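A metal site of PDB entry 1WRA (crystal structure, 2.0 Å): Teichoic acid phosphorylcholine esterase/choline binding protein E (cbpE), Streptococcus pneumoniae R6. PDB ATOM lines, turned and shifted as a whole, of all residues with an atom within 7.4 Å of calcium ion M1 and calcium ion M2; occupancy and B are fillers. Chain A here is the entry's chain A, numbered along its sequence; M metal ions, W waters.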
ATOM      1  N   THR A  33     -28.713  15.560  30.778  1.00  0.00           N
ATOM      2  CA  THR A  33     -27.981  16.189  31.914  1.00  0.00           C
ATOM      3  C   THR A  33     -28.071  17.682  31.978  1.00  0.00           C
ATOM      4  O   THR A  33     -27.557  18.291  32.912  1.00  0.00           O
ATOM      5  CB  THR A  33     -26.478  15.823  31.909  1.00  0.00           C
ATOM      6  OG1 THR A  33     -25.821  16.371  30.728  1.00  0.00           O
ATOM      7  CG2 THR A  33     -26.295  14.347  31.867  1.00  0.00           C
ATOM      8  N   GLY A  34     -28.718  18.275  30.988  1.00  0.00           N
ATOM      9  CA  GLY A  34     -28.978  19.698  30.989  1.00  0.00           C
ATOM     10  C   GLY A  34     -27.830  20.528  30.479  1.00  0.00           C
ATOM     11  O   GLY A  34     -26.720  20.032  30.331  1.00  0.00           O
ATOM     12  N   GLU A  35     -28.124  21.801  30.219  1.00  0.00           N
ATOM     13  CA  GLU A  35     -27.188  22.794  29.754  1.00  0.00           C
ATOM     14  C   GLU A  35     -26.199  23.132  30.888  1.00  0.00           C
ATOM     15  O   GLU A  35     -26.591  23.153  32.071  1.00  0.00           O
ATOM     16  CB  GLU A  35     -27.951  24.075  29.369  1.00  0.00           C
ATOM     17  CG  GLU A  35     -27.080  25.212  28.838  1.00  0.00           C
ATOM     18  CD  GLU A  35     -26.377  24.810  27.548  1.00  0.00           C
ATOM     19  OE1 GLU A  35     -27.074  24.752  26.493  1.00  0.00           O
ATOM     20  OE2 GLU A  35     -25.162  24.460  27.621  1.00  0.00           O
ATOM     21  N   ASP A  36     -24.944  23.369  30.517  1.00  0.00           N
ATOM     22  CA  ASP A  36     -23.852  23.670  31.434  1.00  0.00           C
ATOM     23  C   ASP A  36     -23.277  25.079  31.236  1.00  0.00           C
ATOM     24  O   ASP A  36     -23.423  25.673  30.160  1.00  0.00           O
ATOM     25  CB  ASP A  36     -22.745  22.615  31.278  1.00  0.00           C
ATOM     26  CG  ASP A  36     -21.970  22.722  29.963  1.00  0.00           C
ATOM     27  OD1 ASP A  36     -22.561  23.087  28.899  1.00  0.00           O
ATOM     28  OD2 ASP A  36     -20.758  22.374  29.920  1.00  0.00           O
ATOM     29  N   TYR A  37     -22.609  25.613  32.268  1.00  0.00           N
ATOM     30  CA  TYR A  37     -21.927  26.918  32.192  1.00  0.00           C
ATOM     31  C   TYR A  37     -20.894  27.017  31.060  1.00  0.00           C
ATOM     32  O   TYR A  37     -20.805  28.036  30.375  1.00  0.00           O
ATOM     33  CB  TYR A  37     -21.211  27.251  33.524  1.00  0.00           C
ATOM     34  CG  TYR A  37     -22.186  27.488  34.619  1.00  0.00           C
ATOM     35  CD1 TYR A  37     -23.007  28.616  34.591  1.00  0.00           C
ATOM     36  CD2 TYR A  37     -22.336  26.597  35.653  1.00  0.00           C
ATOM     37  CE1 TYR A  37     -23.912  28.868  35.582  1.00  0.00           C
ATOM     38  CE2 TYR A  37     -23.285  26.842  36.662  1.00  0.00           C
ATOM     39  CZ  TYR A  37     -24.062  27.965  36.608  1.00  0.00           C
ATOM     40  OH  TYR A  37     -24.992  28.243  37.570  1.00  0.00           O
ATOM     41  N   ASP A  38     -20.144  25.953  30.875  1.00  0.00           N
ATOM     42  CA  ASP A  38     -19.020  25.974  29.929  1.00  0.00           C
ATOM     43  C   ASP A  38     -19.543  26.012  28.471  1.00  0.00           C
ATOM     44  O   ASP A  38     -20.699  25.673  28.194  1.00  0.00           O
ATOM     45  CB  ASP A  38     -18.137  24.747  30.258  1.00  0.00           C
ATOM     46  CG  ASP A  38     -16.835  24.701  29.513  1.00  0.00           C
ATOM     47  OD1 ASP A  38     -16.280  25.752  29.159  1.00  0.00           O
ATOM     48  OD2 ASP A  38     -16.306  23.598  29.228  1.00  0.00           O
ATOM     49  N   PHE A  39     -18.688  26.489  27.574  1.00  0.00           N
ATOM     50  CA  PHE A  39     -18.916  26.503  26.136  1.00  0.00           C
ATOM     51  C   PHE A  39     -17.589  26.890  25.513  1.00  0.00           C
ATOM     52  O   PHE A  39     -16.754  27.538  26.152  1.00  0.00           O
ATOM     53  CB  PHE A  39     -20.005  27.526  25.726  1.00  0.00           C
ATOM     54  CG  PHE A  39     -19.757  28.945  26.177  1.00  0.00           C
ATOM     55  CD1 PHE A  39     -19.039  29.837  25.389  1.00  0.00           C
ATOM     56  CD2 PHE A  39     -20.309  29.432  27.367  1.00  0.00           C
ATOM     57  CE1 PHE A  39     -18.856  31.149  25.779  1.00  0.00           C
ATOM     58  CE2 PHE A  39     -20.122  30.749  27.749  1.00  0.00           C
ATOM     59  CZ  PHE A  39     -19.393  31.616  26.936  1.00  0.00           C
ATOM     60  N   PRO A  40     -17.371  26.514  24.271  1.00  0.00           N
ATOM     61  CA  PRO A  40     -16.111  26.910  23.628  1.00  0.00           C
ATOM     62  C   PRO A  40     -16.173  28.368  23.165  1.00  0.00           C
ATOM     63  O   PRO A  40     -17.210  28.831  22.689  1.00  0.00           O
ATOM     64  CB  PRO A  40     -16.046  25.978  22.436  1.00  0.00           C
ATOM     65  CG  PRO A  40     -17.535  25.739  22.048  1.00  0.00           C
ATOM     66  CD  PRO A  40     -18.248  25.710  23.366  1.00  0.00           C
ATOM     67  N   ILE A  53     -24.304  29.413  19.713  1.00  0.00           N
ATOM     68  CA  ILE A  53     -23.763  28.629  20.822  1.00  0.00           C
ATOM     69  C   ILE A  53     -24.304  29.242  22.118  1.00  0.00           C
ATOM     70  O   ILE A  53     -24.250  30.416  22.322  1.00  0.00           O
ATOM     71  CB  ILE A  53     -22.225  28.649  20.831  1.00  0.00           C
ATOM     72  CG1 ILE A  53     -21.683  27.738  19.698  1.00  0.00           C
ATOM     73  CG2 ILE A  53     -21.685  28.248  22.234  1.00  0.00           C
ATOM     74  CD1 ILE A  53     -20.150  27.666  19.602  1.00  0.00           C
ATOM     75  N   GLU A  54     -24.809  28.413  22.994  1.00  0.00           N
ATOM     76  CA  GLU A  54     -25.365  28.929  24.216  1.00  0.00           C
ATOM     77  C   GLU A  54     -24.398  29.368  25.323  1.00  0.00           C
ATOM     78  O   GLU A  54     -23.396  28.703  25.567  1.00  0.00           O
ATOM     79  CB  GLU A  54     -26.208  27.828  24.872  1.00  0.00           C
ATOM     80  CG  GLU A  54     -26.850  28.203  26.219  1.00  0.00           C
ATOM     81  CD  GLU A  54     -27.935  29.218  25.997  1.00  0.00           C
ATOM     82  OE1 GLU A  54     -27.700  30.437  26.187  1.00  0.00           O
ATOM     83  OE2 GLU A  54     -29.000  28.792  25.541  1.00  0.00           O
ATOM     84  N   THR A  55     -24.675  30.504  25.935  1.00  0.00           N
ATOM     85  CA  THR A  55     -23.714  31.344  26.667  1.00  0.00           C
ATOM     86  C   THR A  55     -24.504  31.804  27.952  1.00  0.00           C
ATOM     87  O   THR A  55     -23.914  32.110  28.986  1.00  0.00           O
ATOM     88  CB  THR A  55     -23.076  32.532  25.941  1.00  0.00           C
ATOM     89  OG1 THR A  55     -24.067  33.528  25.665  1.00  0.00           O
ATOM     90  CG2 THR A  55     -22.424  32.085  24.625  1.00  0.00           C
ATOM     91  N   SER A  56     -25.848  31.828  27.882  1.00  0.00           N
ATOM     92  CA  SER A  56     -26.639  32.424  28.955  1.00  0.00           C
ATOM     93  C   SER A  56     -26.801  31.568  30.226  1.00  0.00           C
ATOM     94  O   SER A  56     -27.329  30.440  30.192  1.00  0.00           O
ATOM     95  CB  SER A  56     -27.999  32.873  28.433  1.00  0.00           C
ATOM     96  OG  SER A  56     -28.806  33.385  29.491  1.00  0.00           O
ATOM     97  N   VAL A  60     -28.818  27.642  32.021  1.00  0.00           N
ATOM     98  CA  VAL A  60     -27.956  26.614  32.596  1.00  0.00           C
ATOM     99  C   VAL A  60     -28.673  25.813  33.679  1.00  0.00           C
ATOM    100  O   VAL A  60     -29.312  26.378  34.545  1.00  0.00           O
ATOM    101  CB  VAL A  60     -26.639  27.243  33.152  1.00  0.00           C
ATOM    102  CG1 VAL A  60     -25.867  26.266  33.985  1.00  0.00           C
ATOM    103  CG2 VAL A  60     -25.781  27.710  32.006  1.00  0.00           C
ATOM    104  N   THR A  62     -26.911  23.211  35.410  1.00  0.00           N
ATOM    105  CA  THR A  62     -25.858  22.656  36.250  1.00  0.00           C
ATOM    106  C   THR A  62     -26.182  22.660  37.729  1.00  0.00           C
ATOM    107  O   THR A  62     -26.091  21.622  38.369  1.00  0.00           O
ATOM    108  CB  THR A  62     -24.548  23.409  36.018  1.00  0.00           C
ATOM    109  OG1 THR A  62     -24.208  23.350  34.635  1.00  0.00           O
ATOM    110  CG2 THR A  62     -23.381  22.711  36.751  1.00  0.00           C
ATOM    111  N   SER A  87     -25.895  20.976  23.508  1.00  0.00           N
ATOM    112  CA  SER A  87     -25.367  21.387  24.809  1.00  0.00           C
ATOM    113  C   SER A  87     -26.410  21.354  25.931  1.00  0.00           C
ATOM    114  O   SER A  87     -26.080  21.053  27.105  1.00  0.00           O
ATOM    115  CB  SER A  87     -24.782  22.799  24.681  1.00  0.00           C
ATOM    116  OG  SER A  87     -25.784  23.769  24.305  1.00  0.00           O
ATOM    117  N   ASP A  88     -27.665  21.641  25.581  1.00  0.00           N
ATOM    118  CA  ASP A  88     -28.773  21.630  26.552  1.00  0.00           C
ATOM    119  C   ASP A  88     -29.254  20.207  26.931  1.00  0.00           C
ATOM    120  O   ASP A  88     -30.232  20.027  27.681  1.00  0.00           O
ATOM    121  CB  ASP A  88     -29.938  22.524  26.060  1.00  0.00           C
ATOM    122  CG  ASP A  88     -30.526  22.057  24.735  1.00  0.00           C
ATOM    123  OD1 ASP A  88     -29.787  22.027  23.707  1.00  0.00           O
ATOM    124  OD2 ASP A  88     -31.717  21.680  24.662  1.00  0.00           O
ATOM    125  N   ILE A  90     -26.363  17.291  26.586  1.00  0.00           N
ATOM    126  CA  ILE A  90     -25.085  16.639  26.908  1.00  0.00           C
ATOM    127  C   ILE A  90     -24.234  17.492  27.850  1.00  0.00           C
ATOM    128  O   ILE A  90     -23.211  17.049  28.359  1.00  0.00           O
ATOM    129  CB  ILE A  90     -24.322  16.375  25.609  1.00  0.00           C
ATOM    130  CG1 ILE A  90     -23.339  15.211  25.777  1.00  0.00           C
ATOM    131  CG2 ILE A  90     -23.579  17.657  25.130  1.00  0.00           C
ATOM    132  CD1 ILE A  90     -22.749  14.750  24.439  1.00  0.00           C
ATOM    133  N   GLY A  91     -24.690  18.714  28.093  1.00  0.00           N
ATOM    134  CA  GLY A  91     -23.868  19.713  28.742  1.00  0.00           C
ATOM    135  C   GLY A  91     -23.185  19.317  30.037  1.00  0.00           C
ATOM    136  O   GLY A  91     -22.016  19.620  30.178  1.00  0.00           O
ATOM    137  N   ASN A  92     -23.881  18.694  30.984  1.00  0.00           N
ATOM    138  CA  ASN A  92     -23.283  18.385  32.281  1.00  0.00           C
ATOM    139  C   ASN A  92     -22.660  16.980  32.397  1.00  0.00           C
ATOM    140  O   ASN A  92     -22.323  16.517  33.497  1.00  0.00           O
ATOM    141  CB  ASN A  92     -24.268  18.629  33.415  1.00  0.00           C
ATOM    142  CG  ASN A  92     -24.551  20.112  33.628  1.00  0.00           C
ATOM    143  OD1 ASN A  92     -23.667  20.895  34.034  1.00  0.00           O
ATOM    144  ND2 ASN A  92     -25.805  20.510  33.355  1.00  0.00           N
ATOM    145  N   VAL A  93     -22.481  16.295  31.267  1.00  0.00           N
ATOM    146  CA  VAL A  93     -21.981  14.930  31.363  1.00  0.00           C
ATOM    147  C   VAL A  93     -20.561  14.851  31.937  1.00  0.00           C
ATOM    148  O   VAL A  93     -20.310  14.011  32.816  1.00  0.00           O
ATOM    149  CB  VAL A  93     -22.010  14.193  30.028  1.00  0.00           C
ATOM    150  CG1 VAL A  93     -21.329  12.822  30.138  1.00  0.00           C
ATOM    151  CG2 VAL A  93     -23.456  13.966  29.601  1.00  0.00           C
ATOM    152  N   ASP A  94     -19.627  15.641  31.405  1.00  0.00           N
ATOM    153  CA  ASP A  94     -18.239  15.596  31.901  1.00  0.00           C
ATOM    154  C   ASP A  94     -18.109  16.073  33.375  1.00  0.00           C
ATOM    155  O   ASP A  94     -17.302  15.553  34.132  1.00  0.00           O
ATOM    156  CB  ASP A  94     -17.264  16.378  30.994  1.00  0.00           C
ATOM    157  CG  ASP A  94     -17.654  17.850  30.824  1.00  0.00           C
ATOM    158  OD1 ASP A  94     -18.776  18.149  30.355  1.00  0.00           O
ATOM    159  OD2 ASP A  94     -16.912  18.788  31.104  1.00  0.00           O
ATOM    160  N   GLU A  95     -18.914  17.050  33.760  1.00  0.00           N
ATOM    161  CA  GLU A  95     -18.987  17.451  35.180  1.00  0.00           C
ATOM    162  C   GLU A  95     -19.484  16.306  36.055  1.00  0.00           C
ATOM    163  O   GLU A  95     -19.002  16.120  37.175  1.00  0.00           O
ATOM    164  CB  GLU A  95     -19.874  18.692  35.384  1.00  0.00           C
ATOM    165  CG  GLU A  95     -19.313  20.006  34.807  1.00  0.00           C
ATOM    166  CD  GLU A  95     -19.591  20.197  33.294  1.00  0.00           C
ATOM    167  OE1 GLU A  95     -20.266  19.374  32.660  1.00  0.00           O
ATOM    168  OE2 GLU A  95     -19.098  21.165  32.704  1.00  0.00           O
ATOM    169  N   LEU A  96     -20.469  15.543  35.573  1.00  0.00           N
ATOM    170  CA  LEU A  96     -20.997  14.415  36.332  1.00  0.00           C
ATOM    171  C   LEU A  96     -19.931  13.323  36.403  1.00  0.00           C
ATOM    172  O   LEU A  96     -19.721  12.737  37.471  1.00  0.00           O
ATOM    173  CB  LEU A  96     -22.312  13.868  35.707  1.00  0.00           C
ATOM    174  CG  LEU A  96     -23.534  14.770  35.929  1.00  0.00           C
ATOM    175  CD1 LEU A  96     -24.750  14.486  34.962  1.00  0.00           C
ATOM    176  CD2 LEU A  96     -24.036  14.729  37.384  1.00  0.00           C
ATOM    177  N   ASP A 123     -21.877  23.917  19.146  1.00  0.00           N
ATOM    178  CA  ASP A 123     -21.242  23.434  20.311  1.00  0.00           C
ATOM    179  C   ASP A 123     -21.149  21.894  20.369  1.00  0.00           C
ATOM    180  O   ASP A 123     -20.661  21.288  21.338  1.00  0.00           O
ATOM    181  CB  ASP A 123     -22.269  23.882  21.508  1.00  0.00           C
ATOM    182  CG  ASP A 123     -21.506  24.339  22.535  1.00  0.00           C
ATOM    183  OD1 ASP A 123     -20.335  24.356  22.015  1.00  0.00           O
ATOM    184  OD2 ASP A 123     -21.743  24.566  23.717  1.00  0.00           O
ATOM    185  N   TYR A 126     -17.792  19.840  20.784  1.00  0.00           N
ATOM    186  CA  TYR A 126     -17.139  20.158  22.043  1.00  0.00           C
ATOM    187  C   TYR A 126     -17.749  19.307  23.170  1.00  0.00           C
ATOM    188  O   TYR A 126     -17.036  18.665  23.959  1.00  0.00           O
ATOM    189  CB  TYR A 126     -17.286  21.645  22.324  1.00  0.00           C
ATOM    190  CG  TYR A 126     -16.611  22.118  23.585  1.00  0.00           C
ATOM    191  CD1 TYR A 126     -17.336  22.431  24.702  1.00  0.00           C
ATOM    192  CD2 TYR A 126     -15.225  22.281  23.623  1.00  0.00           C
ATOM    193  CE1 TYR A 126     -16.706  22.859  25.862  1.00  0.00           C
ATOM    194  CE2 TYR A 126     -14.588  22.720  24.768  1.00  0.00           C
ATOM    195  CZ  TYR A 126     -15.346  23.014  25.884  1.00  0.00           C
ATOM    196  OH  TYR A 126     -14.731  23.491  27.022  1.00  0.00           O
ATOM    197  N   GLY A 127     -19.069  19.274  23.223  1.00  0.00           N
ATOM    198  CA  GLY A 127     -19.777  18.443  24.186  1.00  0.00           C
ATOM    199  C   GLY A 127     -19.563  16.934  24.069  1.00  0.00           C
ATOM    200  O   GLY A 127     -19.329  16.275  25.070  1.00  0.00           O
ATOM    201  N   LYS A 130     -15.970  16.153  25.085  1.00  0.00           N
ATOM    202  CA  LYS A 130     -15.915  16.186  26.552  1.00  0.00           C
ATOM    203  C   LYS A 130     -16.373  14.875  27.185  1.00  0.00           C
ATOM    204  O   LYS A 130     -15.803  14.420  28.177  1.00  0.00           O
ATOM    205  CB  LYS A 130     -16.738  17.351  27.139  1.00  0.00           C
ATOM    206  CG  LYS A 130     -16.030  18.710  27.073  1.00  0.00           C
ATOM    207  CD  LYS A 130     -14.961  18.833  28.164  1.00  0.00           C
ATOM    208  CE  LYS A 130     -14.176  20.130  28.033  1.00  0.00           C
ATOM    209  NZ  LYS A 130     -13.104  20.235  29.049  1.00  0.00           N
HETATM  210 CA    CA M   1     -22.918  25.116  27.710  1.00  0.00          CA
HETATM  211 CA    CA M   2     -19.742  20.329  30.342  1.00  0.00          CA
HETATM  212  O   HOH W   1     -17.568  21.140  29.718  1.00  0.00           O
HETATM  213  O   HOH W   2     -19.997  19.737  27.880  1.00  0.00           O
HETATM  214  O   HOH W   3     -23.021  25.987  25.513  1.00  0.00           O
HETATM  215  O   HOH W   4     -21.691  23.595  26.069  1.00  0.00           O
HETATM  216  O   HOH W   5     -23.534  27.351  27.897  1.00  0.00           O
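Calcium ion M1 is bound by water W5 (2.3 Å), the backbone carbonyl oxygen (O) of Asp 38 (2.3 Å), the side-chain carboxylate (OE2) of Glu 35 (2.3 Å), water W3 (2.4 Å), the side-chain carboxylate (OD1) of Asp 36 (2.4 Å), water W4 (2.6 Å) and the backbone carbonyl oxygen (O) of Asp 36 (2.6 Å).
The side-chain carboxylate (OD2) of Asp 36 is bound to calcium ion M2, 2.3 Å away. OD1 of Asp 94 is bound to calcium ion M2 (2.4 Å). O of Gly 91 is bound to calcium ion M2, at 2.4 Å. Water W1 is bound to calcium ion M2, at 2.4 Å. Water W2 is bound to calcium ion M2. Calcium ion M2 is bound by OE1 of Glu 95 (2.6 Å). Calcium ion M2 is bound by OE2 of Glu 95, at 2.6 Å.
Of the 27 residues printed, 3 come within 4 Å of calcium ion M1.
Water W3 lies within hydrogen-bond range of OD2 of Asp 123 and O of Glu 54. Water W1 bridges the side-chain carboxylate (OD2) of Asp 38 and the side-chain carboxylate (OD2) of Asp 94.
OE1 of Glu 35 is in hydrogen-bond range of N of Asp 88, at 3.3 Å. OD2 of Asp 38 is in hydrogen-bond range of OH of Tyr 126. The backbone carbonyl oxygen (O) of Glu 35 lies within hydrogen-bond range of the backbone NH (N) of Thr 62 (3.4 Å). The side-chain carboxylate (OE1) of Glu 35 lies within hydrogen-bond range of the side-chain hydroxyl (OG) of Ser 87, at 2.7 Å. The backbone NH of Gly 91 sits close to the backbone carbonyl oxygen of Gly 34 (3.3 Å). ND2 of Asn 92 lies within hydrogen-bond range of O of Glu 35 (3.0 Å).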
